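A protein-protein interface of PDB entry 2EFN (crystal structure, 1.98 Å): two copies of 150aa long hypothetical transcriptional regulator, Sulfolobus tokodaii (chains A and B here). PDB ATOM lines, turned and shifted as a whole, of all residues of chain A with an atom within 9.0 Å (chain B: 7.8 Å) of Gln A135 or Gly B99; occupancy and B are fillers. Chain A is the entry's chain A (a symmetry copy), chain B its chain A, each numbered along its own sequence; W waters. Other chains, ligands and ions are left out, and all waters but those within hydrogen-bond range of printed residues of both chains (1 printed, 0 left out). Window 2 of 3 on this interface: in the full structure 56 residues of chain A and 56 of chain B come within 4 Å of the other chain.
Gln A135 touches just these residues of chain B: Val B97, Leu B98, Gly B99 and Asp B100. Of the printed residues of chain B, Lys A139 touches Phe B96. Printed residues of chain A within 4 Å of Val B97: Gln A135, Val A136 and Val A137. Asp B100 touches one residue of chain A. The nearest printed residue of chain A that does not touch Phe B96 is Val A136 (4.1 Å).
CD1 of Ile B104 touches CD1 of Ile A66 (3.7 Å). Gln A135 touches Val B97 (OE1 to CG2, 3.5 Å). Gln A135 touches Gly B99 (OE1 to C, 3.5 Å). CA of Val B97 touches O of Val A136, at 3.2 Å. Val A137 touches Phe B96. CG2 of Val A137 touches CG1 of Val B97, 3.7 Å away. Val A138 touches Leu B98 (CG1 to CD1, 3.5 Å).
O of Phe B96 sits at hydrogen-bond distance from N of Val A138, at 3.0 Å. N of Leu B98 is in hydrogen-bond range of O of Val A136 (2.8 Å). N of Phe B96 lies within hydrogen-bond range of O of Lys A139 (2.9 Å). The side-chain amide oxygen (OE1) of Gln A135 sits close to the backbone carbonyl oxygen (O) of Leu B98 (2.9 Å). OE1 of Gln A135 is in hydrogen-bond range of N of Asp B100 (2.6 Å).
The backbone NH (N) of Val B97 lies within hydrogen-bond range of the backbone carbonyl oxygen (O) of Asp B102 (2.8 Å). The backbone NH of Gln A135 sits at hydrogen-bond distance from the backbone carbonyl oxygen of Ile A66 (2.7 Å). The backbone carbonyl oxygen of Ile A64 sits at hydrogen-bond distance from the backbone NH of Val A137 (2.9 Å). NE2 of Gln A135 lies within hydrogen-bond range of OG of Ser A133 (3.1 Å). N of Gly B99 lies close to ND2 of Asn B101, 2.9 Å away.
Water W1 lies within hydrogen-bond range of NE2 of Gln A135 (2.6 Å), OD1 of Asp B100 (2.8 Å) and OG of Ser A133 (3.5 Å).
Printed residues of chain A that touch a printed residue of chain B: Ile A66, Gln A135, Val A136, Val A137, Val A138 and Lys A139. Hydrophobic or aromatic side chains of chain A within 4 Å of the printed part of chain B: Ile A66, Val A137 and Val A138. Among the printed residues, no Asp or Glu carboxylate lies within 4 Å of a Lys or Arg side-chain nitrogen of the other chain.
Positions printed for both chains: 68, 100 and 104.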
ATOM      1  N   TYR A  63      17.514 -25.266 -16.285  1.00  0.00           N
ATOM      2  CA  TYR A  63      18.929 -24.942 -16.441  1.00  0.00           C
ATOM      3  C   TYR A  63      19.730 -25.571 -15.307  1.00  0.00           C
ATOM      4  O   TYR A  63      19.852 -25.002 -14.220  1.00  0.00           O
ATOM      5  CB  TYR A  63      19.118 -23.425 -16.445  1.00  0.00           C
ATOM      6  CG  TYR A  63      20.113 -22.943 -17.478  1.00  0.00           C
ATOM      7  CD1 TYR A  63      19.778 -22.912 -18.834  1.00  0.00           C
ATOM      8  CD2 TYR A  63      21.395 -22.541 -17.106  1.00  0.00           C
ATOM      9  CE1 TYR A  63      20.695 -22.488 -19.794  1.00  0.00           C
ATOM     10  CE2 TYR A  63      22.324 -22.116 -18.057  1.00  0.00           C
ATOM     11  CZ  TYR A  63      21.965 -22.091 -19.400  1.00  0.00           C
ATOM     12  OH  TYR A  63      22.864 -21.651 -20.340  1.00  0.00           O
ATOM     13  N   ILE A  64      20.268 -26.754 -15.584  1.00  0.00           N
ATOM     14  CA  ILE A  64      21.035 -27.528 -14.615  1.00  0.00           C
ATOM     15  C   ILE A  64      22.519 -27.402 -14.928  1.00  0.00           C
ATOM     16  O   ILE A  64      22.943 -27.604 -16.070  1.00  0.00           O
ATOM     17  CB  ILE A  64      20.609 -29.010 -14.675  1.00  0.00           C
ATOM     18  CG1 ILE A  64      19.079 -29.106 -14.619  1.00  0.00           C
ATOM     19  CG2 ILE A  64      21.221 -29.787 -13.516  1.00  0.00           C
ATOM     20  CD1 ILE A  64      18.449 -28.385 -13.434  1.00  0.00           C
ATOM     21  N   VAL A  65      23.307 -27.069 -13.913  1.00  0.00           N
ATOM     22  CA  VAL A  65      24.738 -26.874 -14.108  1.00  0.00           C
ATOM     23  C   VAL A  65      25.621 -27.507 -13.044  1.00  0.00           C
ATOM     24  O   VAL A  65      25.214 -27.674 -11.888  1.00  0.00           O
ATOM     25  CB  VAL A  65      25.083 -25.364 -14.155  1.00  0.00           C
ATOM     26  CG1 VAL A  65      24.508 -24.732 -15.411  1.00  0.00           C
ATOM     27  CG2 VAL A  65      24.514 -24.666 -12.922  1.00  0.00           C
ATOM     28  N   ILE A  66      26.834 -27.857 -13.464  1.00  0.00           N
ATOM     29  CA  ILE A  66      27.855 -28.438 -12.598  1.00  0.00           C
ATOM     30  C   ILE A  66      29.086 -27.573 -12.855  1.00  0.00           C
ATOM     31  O   ILE A  66      29.602 -27.548 -13.970  1.00  0.00           O
ATOM     32  CB  ILE A  66      28.165 -29.892 -12.986  1.00  0.00           C
ATOM     33  CG1 ILE A  66      26.915 -30.761 -12.777  1.00  0.00           C
ATOM     34  CG2 ILE A  66      29.349 -30.403 -12.168  1.00  0.00           C
ATOM     35  CD1 ILE A  66      27.068 -32.211 -13.256  1.00  0.00           C
ATOM     36  N   THR A  67      29.550 -26.865 -11.831  1.00  0.00           N
ATOM     37  CA  THR A  67      30.685 -25.965 -12.006  1.00  0.00           C
ATOM     38  C   THR A  67      31.909 -26.275 -11.158  1.00  0.00           C
ATOM     39  O   THR A  67      31.798 -26.536  -9.958  1.00  0.00           O
ATOM     40  CB  THR A  67      30.272 -24.499 -11.706  1.00  0.00           C
ATOM     41  OG1 THR A  67      29.175 -24.118 -12.544  1.00  0.00           O
ATOM     42  CG2 THR A  67      31.436 -23.554 -11.949  1.00  0.00           C
ATOM     43  N   SER A  68      33.074 -26.229 -11.792  1.00  0.00           N
ATOM     44  CA  SER A  68      34.336 -26.447 -11.099  1.00  0.00           C
ATOM     45  C   SER A  68      34.863 -25.067 -10.734  1.00  0.00           C
ATOM     46  O   SER A  68      34.931 -24.177 -11.585  1.00  0.00           O
ATOM     47  CB  SER A  68      35.339 -27.161 -12.005  1.00  0.00           C
ATOM     48  OG  SER A  68      35.025 -28.540 -12.104  1.00  0.00           O
ATOM     49  N   ASP A 100      41.488 -32.599  -9.526  1.00  0.00           N
ATOM     50  CA  ASP A 100      41.436 -31.206  -9.970  1.00  0.00           C
ATOM     51  C   ASP A 100      41.730 -30.327  -8.754  1.00  0.00           C
ATOM     52  O   ASP A 100      41.958 -29.125  -8.886  1.00  0.00           O
ATOM     53  CB  ASP A 100      40.048 -30.830 -10.511  1.00  0.00           C
ATOM     54  CG  ASP A 100      39.735 -31.471 -11.859  1.00  0.00           C
ATOM     55  OD1 ASP A 100      40.678 -31.836 -12.592  1.00  0.00           O
ATOM     56  OD2 ASP A 100      38.532 -31.586 -12.190  1.00  0.00           O
ATOM     57  N   ILE A 104      33.488 -28.637  -6.677  1.00  0.00           N
ATOM     58  CA  ILE A 104      32.535 -29.001  -7.718  1.00  0.00           C
ATOM     59  C   ILE A 104      31.194 -28.590  -7.127  1.00  0.00           C
ATOM     60  O   ILE A 104      30.819 -29.057  -6.048  1.00  0.00           O
ATOM     61  CB  ILE A 104      32.536 -30.505  -8.034  1.00  0.00           C
ATOM     62  CG1 ILE A 104      33.851 -30.879  -8.735  1.00  0.00           C
ATOM     63  CG2 ILE A 104      31.333 -30.849  -8.919  1.00  0.00           C
ATOM     64  CD1 ILE A 104      33.910 -32.313  -9.247  1.00  0.00           C
ATOM     65  N   VAL A 105      30.492 -27.714  -7.841  1.00  0.00           N
ATOM     66  CA  VAL A 105      29.210 -27.161  -7.402  1.00  0.00           C
ATOM     67  C   VAL A 105      28.028 -27.587  -8.268  1.00  0.00           C
ATOM     68  O   VAL A 105      28.020 -27.330  -9.470  1.00  0.00           O
ATOM     69  CB  VAL A 105      29.281 -25.610  -7.422  1.00  0.00           C
ATOM     70  CG1 VAL A 105      27.975 -25.002  -6.906  1.00  0.00           C
ATOM     71  CG2 VAL A 105      30.473 -25.141  -6.591  1.00  0.00           C
ATOM     72  N   MET A 106      27.029 -28.208  -7.643  1.00  0.00           N
ATOM     73  CA  MET A 106      25.820 -28.661  -8.337  1.00  0.00           C
ATOM     74  C   MET A 106      24.727 -27.633  -8.075  1.00  0.00           C
ATOM     75  O   MET A 106      24.497 -27.257  -6.923  1.00  0.00           O
ATOM     76  CB  MET A 106      25.348 -30.006  -7.783  1.00  0.00           C
ATOM     77  CG  MET A 106      26.451 -31.008  -7.485  1.00  0.00           C
ATOM     78  SD  MET A 106      27.238 -31.629  -8.966  1.00  0.00           S
ATOM     79  CE  MET A 106      25.990 -32.763  -9.536  1.00  0.00           C
ATOM     80  N   ALA A 107      24.048 -27.190  -9.130  1.00  0.00           N
ATOM     81  CA  ALA A 107      22.988 -26.199  -8.977  1.00  0.00           C
ATOM     82  C   ALA A 107      21.893 -26.376 -10.013  1.00  0.00           C
ATOM     83  O   ALA A 107      22.085 -27.034 -11.040  1.00  0.00           O
ATOM     84  CB  ALA A 107      23.570 -24.790  -9.073  1.00  0.00           C
ATOM     85  N   PHE A 115      20.270 -18.338 -13.837  1.00  0.00           N
ATOM     86  CA  PHE A 115      21.602 -18.876 -13.582  1.00  0.00           C
ATOM     87  C   PHE A 115      22.627 -17.744 -13.565  1.00  0.00           C
ATOM     88  O   PHE A 115      23.472 -17.669 -12.677  1.00  0.00           O
ATOM     89  CB  PHE A 115      21.996 -19.879 -14.675  1.00  0.00           C
ATOM     90  CG  PHE A 115      23.476 -20.164 -14.728  1.00  0.00           C
ATOM     91  CD1 PHE A 115      24.098 -20.886 -13.715  1.00  0.00           C
ATOM     92  CD2 PHE A 115      24.252 -19.691 -15.782  1.00  0.00           C
ATOM     93  CE1 PHE A 115      25.474 -21.131 -13.751  1.00  0.00           C
ATOM     94  CE2 PHE A 115      25.629 -19.931 -15.823  1.00  0.00           C
ATOM     95  CZ  PHE A 115      26.235 -20.652 -14.809  1.00  0.00           C
ATOM     96  N   PHE A 119      23.755 -17.149  -9.860  1.00  0.00           N
ATOM     97  CA  PHE A 119      24.994 -17.885  -9.668  1.00  0.00           C
ATOM     98  C   PHE A 119      26.248 -17.289 -10.291  1.00  0.00           C
ATOM     99  O   PHE A 119      27.124 -16.794  -9.581  1.00  0.00           O
ATOM    100  CB  PHE A 119      24.813 -19.323 -10.162  1.00  0.00           C
ATOM    101  CG  PHE A 119      25.997 -20.203  -9.904  1.00  0.00           C
ATOM    102  CD1 PHE A 119      27.001 -20.342 -10.860  1.00  0.00           C
ATOM    103  CD2 PHE A 119      26.135 -20.861  -8.684  1.00  0.00           C
ATOM    104  CE1 PHE A 119      28.126 -21.123 -10.604  1.00  0.00           C
ATOM    105  CE2 PHE A 119      27.263 -21.647  -8.415  1.00  0.00           C
ATOM    106  CZ  PHE A 119      28.257 -21.777  -9.377  1.00  0.00           C
ATOM    107  N   THR A 132      36.896 -20.871 -13.132  1.00  0.00           N
ATOM    108  CA  THR A 132      35.631 -21.584 -13.009  1.00  0.00           C
ATOM    109  C   THR A 132      35.344 -22.201 -14.366  1.00  0.00           C
ATOM    110  O   THR A 132      35.764 -21.676 -15.401  1.00  0.00           O
ATOM    111  CB  THR A 132      34.435 -20.673 -12.643  1.00  0.00           C
ATOM    112  OG1 THR A 132      34.119 -19.828 -13.756  1.00  0.00           O
ATOM    113  CG2 THR A 132      34.755 -19.824 -11.422  1.00  0.00           C
ATOM    114  N   SER A 133      34.647 -23.328 -14.353  1.00  0.00           N
ATOM    115  CA  SER A 133      34.271 -24.012 -15.578  1.00  0.00           C
ATOM    116  C   SER A 133      32.892 -24.595 -15.319  1.00  0.00           C
ATOM    117  O   SER A 133      32.732 -25.477 -14.481  1.00  0.00           O
ATOM    118  CB  SER A 133      35.260 -25.133 -15.911  1.00  0.00           C
ATOM    119  OG  SER A 133      34.823 -25.842 -17.061  1.00  0.00           O
ATOM    120  N   THR A 134      31.901 -24.085 -16.041  1.00  0.00           N
ATOM    121  CA  THR A 134      30.526 -24.532 -15.880  1.00  0.00           C
ATOM    122  C   THR A 134      30.122 -25.500 -16.978  1.00  0.00           C
ATOM    123  O   THR A 134      30.148 -25.155 -18.157  1.00  0.00           O
ATOM    124  CB  THR A 134      29.558 -23.337 -15.910  1.00  0.00           C
ATOM    125  OG1 THR A 134      29.805 -22.502 -14.771  1.00  0.00           O
ATOM    126  CG2 THR A 134      28.103 -23.821 -15.908  1.00  0.00           C
ATOM    127  N   GLN A 135      29.759 -26.711 -16.572  1.00  0.00           N
ATOM    128  CA  GLN A 135      29.319 -27.740 -17.499  1.00  0.00           C
ATOM    129  C   GLN A 135      27.795 -27.702 -17.501  1.00  0.00           C
ATOM    130  O   GLN A 135      27.170 -27.884 -16.459  1.00  0.00           O
ATOM    131  CB  GLN A 135      29.785 -29.111 -17.012  1.00  0.00           C
ATOM    132  CG  GLN A 135      31.271 -29.183 -16.766  1.00  0.00           C
ATOM    133  CD  GLN A 135      32.042 -29.015 -18.043  1.00  0.00           C
ATOM    134  OE1 GLN A 135      31.909 -29.821 -18.963  1.00  0.00           O
ATOM    135  NE2 GLN A 135      32.844 -27.959 -18.121  1.00  0.00           N
ATOM    136  N   VAL A 136      27.197 -27.463 -18.661  1.00  0.00           N
ATOM    137  CA  VAL A 136      25.744 -27.420 -18.730  1.00  0.00           C
ATOM    138  C   VAL A 136      25.162 -28.821 -18.902  1.00  0.00           C
ATOM    139  O   VAL A 136      25.411 -29.491 -19.898  1.00  0.00           O
ATOM    140  CB  VAL A 136      25.273 -26.524 -19.885  1.00  0.00           C
ATOM    141  CG1 VAL A 136      23.754 -26.559 -19.981  1.00  0.00           C
ATOM    142  CG2 VAL A 136      25.771 -25.081 -19.663  1.00  0.00           C
ATOM    143  N   VAL A 137      24.392 -29.261 -17.914  1.00  0.00           N
ATOM    144  CA  VAL A 137      23.758 -30.572 -17.965  1.00  0.00           C
ATOM    145  C   VAL A 137      22.619 -30.530 -18.986  1.00  0.00           C
ATOM    146  O   VAL A 137      21.652 -29.792 -18.822  1.00  0.00           O
ATOM    147  CB  VAL A 137      23.185 -30.964 -16.582  1.00  0.00           C
ATOM    148  CG1 VAL A 137      22.469 -32.317 -16.669  1.00  0.00           C
ATOM    149  CG2 VAL A 137      24.309 -31.017 -15.554  1.00  0.00           C
ATOM    150  N   VAL A 138      22.746 -31.312 -20.050  1.00  0.00           N
ATOM    151  CA  VAL A 138      21.713 -31.344 -21.079  1.00  0.00           C
ATOM    152  C   VAL A 138      20.985 -32.674 -21.058  1.00  0.00           C
ATOM    153  O   VAL A 138      20.103 -32.933 -21.872  1.00  0.00           O
ATOM    154  CB  VAL A 138      22.302 -31.110 -22.486  1.00  0.00           C
ATOM    155  CG1 VAL A 138      22.781 -29.667 -22.613  1.00  0.00           C
ATOM    156  CG2 VAL A 138      23.456 -32.074 -22.735  1.00  0.00           C
ATOM    157  N   LYS A 139      21.351 -33.522 -20.109  1.00  0.00           N
ATOM    158  CA  LYS A 139      20.713 -34.817 -20.004  1.00  0.00           C
ATOM    159  C   LYS A 139      20.962 -35.473 -18.649  1.00  0.00           C
ATOM    160  O   LYS A 139      22.107 -35.673 -18.242  1.00  0.00           O
ATOM    161  CB  LYS A 139      21.217 -35.696 -21.147  1.00  0.00           C
ATOM    162  CG  LYS A 139      21.001 -37.171 -20.953  1.00  0.00           C
ATOM    163  CD  LYS A 139      19.542 -37.569 -21.070  1.00  0.00           C
ATOM    164  CE  LYS A 139      19.218 -38.014 -22.498  1.00  0.00           C
ATOM    165  NZ  LYS A 139      18.155 -39.066 -22.524  1.00  0.00           N
ATOM    166  N   SER B  68      34.503 -38.262 -14.658  1.00  0.00           N
ATOM    167  CA  SER B  68      34.188 -37.778 -15.995  1.00  0.00           C
ATOM    168  C   SER B  68      34.527 -38.916 -16.947  1.00  0.00           C
ATOM    169  O   SER B  68      35.622 -39.479 -16.887  1.00  0.00           O
ATOM    170  CB  SER B  68      35.027 -36.548 -16.340  1.00  0.00           C
ATOM    171  OG  SER B  68      34.518 -35.400 -15.682  1.00  0.00           O
ATOM    172  N   LYS B  70      34.544 -39.958 -21.024  1.00  0.00           N
ATOM    173  CA  LYS B  70      34.401 -39.532 -22.407  1.00  0.00           C
ATOM    174  C   LYS B  70      34.092 -40.743 -23.256  1.00  0.00           C
ATOM    175  O   LYS B  70      34.669 -41.814 -23.056  1.00  0.00           O
ATOM    176  CB  LYS B  70      35.678 -38.850 -22.892  1.00  0.00           C
ATOM    177  CG  LYS B  70      35.925 -37.512 -22.208  1.00  0.00           C
ATOM    178  CD  LYS B  70      37.143 -36.793 -22.758  1.00  0.00           C
ATOM    179  CE  LYS B  70      37.120 -35.325 -22.356  1.00  0.00           C
ATOM    180  NZ  LYS B  70      36.772 -35.166 -20.916  1.00  0.00           N
ATOM    181  N   PHE B  96      24.972 -36.001 -18.751  1.00  0.00           N
ATOM    182  CA  PHE B  96      25.783 -35.709 -19.920  1.00  0.00           C
ATOM    183  C   PHE B  96      25.837 -34.192 -19.895  1.00  0.00           C
ATOM    184  O   PHE B  96      24.806 -33.530 -19.783  1.00  0.00           O
ATOM    185  CB  PHE B  96      25.169 -36.186 -21.233  1.00  0.00           C
ATOM    186  CG  PHE B  96      26.104 -36.021 -22.393  1.00  0.00           C
ATOM    187  CD1 PHE B  96      26.095 -34.858 -23.153  1.00  0.00           C
ATOM    188  CD2 PHE B  96      27.087 -36.976 -22.641  1.00  0.00           C
ATOM    189  CE1 PHE B  96      27.061 -34.641 -24.144  1.00  0.00           C
ATOM    190  CE2 PHE B  96      28.056 -36.769 -23.625  1.00  0.00           C
ATOM    191  CZ  PHE B  96      28.042 -35.593 -24.377  1.00  0.00           C
ATOM    192  N   VAL B  97      27.035 -33.637 -19.990  1.00  0.00           N
ATOM    193  CA  VAL B  97      27.170 -32.193 -19.912  1.00  0.00           C
ATOM    194  C   VAL B  97      27.919 -31.589 -21.085  1.00  0.00           C
ATOM    195  O   VAL B  97      28.741 -32.260 -21.715  1.00  0.00           O
ATOM    196  CB  VAL B  97      27.900 -31.804 -18.607  1.00  0.00           C
ATOM    197  CG1 VAL B  97      27.206 -32.456 -17.416  1.00  0.00           C
ATOM    198  CG2 VAL B  97      29.363 -32.259 -18.660  1.00  0.00           C
ATOM    199  N   LEU B  98      27.623 -30.322 -21.366  1.00  0.00           N
ATOM    200  CA  LEU B  98      28.291 -29.584 -22.426  1.00  0.00           C
ATOM    201  C   LEU B  98      29.546 -28.970 -21.817  1.00  0.00           C
ATOM    202  O   LEU B  98      29.683 -28.924 -20.594  1.00  0.00           O
ATOM    203  CB  LEU B  98      27.378 -28.496 -22.980  1.00  0.00           C
ATOM    204  CG  LEU B  98      26.103 -29.057 -23.605  1.00  0.00           C
ATOM    205  CD1 LEU B  98      25.292 -27.915 -24.205  1.00  0.00           C
ATOM    206  CD2 LEU B  98      26.470 -30.081 -24.683  1.00  0.00           C
ATOM    207  N   GLY B  99      30.453 -28.493 -22.656  1.00  0.00           N
ATOM    208  CA  GLY B  99      31.700 -27.949 -22.142  1.00  0.00           C
ATOM    209  C   GLY B  99      32.700 -29.076 -22.330  1.00  0.00           C
ATOM    210  O   GLY B  99      33.461 -29.084 -23.302  1.00  0.00           O
ATOM    211  N   ASP B 100      32.694 -30.039 -21.412  1.00  0.00           N
ATOM    212  CA  ASP B 100      33.577 -31.199 -21.533  1.00  0.00           C
ATOM    213  C   ASP B 100      32.912 -32.183 -22.496  1.00  0.00           C
ATOM    214  O   ASP B 100      33.535 -33.146 -22.943  1.00  0.00           O
ATOM    215  CB  ASP B 100      33.777 -31.908 -20.184  1.00  0.00           C
ATOM    216  CG  ASP B 100      34.639 -31.113 -19.210  1.00  0.00           C
ATOM    217  OD1 ASP B 100      35.435 -30.260 -19.658  1.00  0.00           O
ATOM    218  OD2 ASP B 100      34.531 -31.366 -17.988  1.00  0.00           O
ATOM    219  N   ASN B 101      31.641 -31.935 -22.807  1.00  0.00           N
ATOM    220  CA  ASN B 101      30.877 -32.808 -23.700  1.00  0.00           C
ATOM    221  C   ASN B 101      31.102 -34.281 -23.369  1.00  0.00           C
ATOM    222  O   ASN B 101      31.543 -35.069 -24.212  1.00  0.00           O
ATOM    223  CB  ASN B 101      31.232 -32.545 -25.172  1.00  0.00           C
ATOM    224  CG  ASN B 101      30.572 -31.286 -25.715  1.00  0.00           C
ATOM    225  OD1 ASN B 101      30.333 -31.163 -26.923  1.00  0.00           O
ATOM    226  ND2 ASN B 101      30.279 -30.341 -24.827  1.00  0.00           N
ATOM    227  N   ASP B 102      30.807 -34.641 -22.124  1.00  0.00           N
ATOM    228  CA  ASP B 102      30.959 -36.015 -21.670  1.00  0.00           C
ATOM    229  C   ASP B 102      30.023 -36.304 -20.507  1.00  0.00           C
ATOM    230  O   ASP B 102      29.175 -35.488 -20.163  1.00  0.00           O
ATOM    231  CB  ASP B 102      32.408 -36.297 -21.253  1.00  0.00           C
ATOM    232  CG  ASP B 102      32.900 -35.379 -20.143  1.00  0.00           C
ATOM    233  OD1 ASP B 102      32.069 -34.813 -19.401  1.00  0.00           O
ATOM    234  OD2 ASP B 102      34.134 -35.244 -20.003  1.00  0.00           O
ATOM    235  N   ILE B 104      29.237 -37.216 -16.476  1.00  0.00           N
ATOM    236  CA  ILE B 104      29.739 -36.979 -15.128  1.00  0.00           C
ATOM    237  C   ILE B 104      28.967 -37.983 -14.284  1.00  0.00           C
ATOM    238  O   ILE B 104      27.733 -37.967 -14.269  1.00  0.00           O
ATOM    239  CB  ILE B 104      29.469 -35.550 -14.630  1.00  0.00           C
ATOM    240  CG1 ILE B 104      30.344 -34.562 -15.416  1.00  0.00           C
ATOM    241  CG2 ILE B 104      29.766 -35.460 -13.129  1.00  0.00           C
ATOM    242  CD1 ILE B 104      30.291 -33.126 -14.909  1.00  0.00           C
HETATM  243  O   HOH W   1      34.586 -27.591 -20.046  1.00  0.00           O
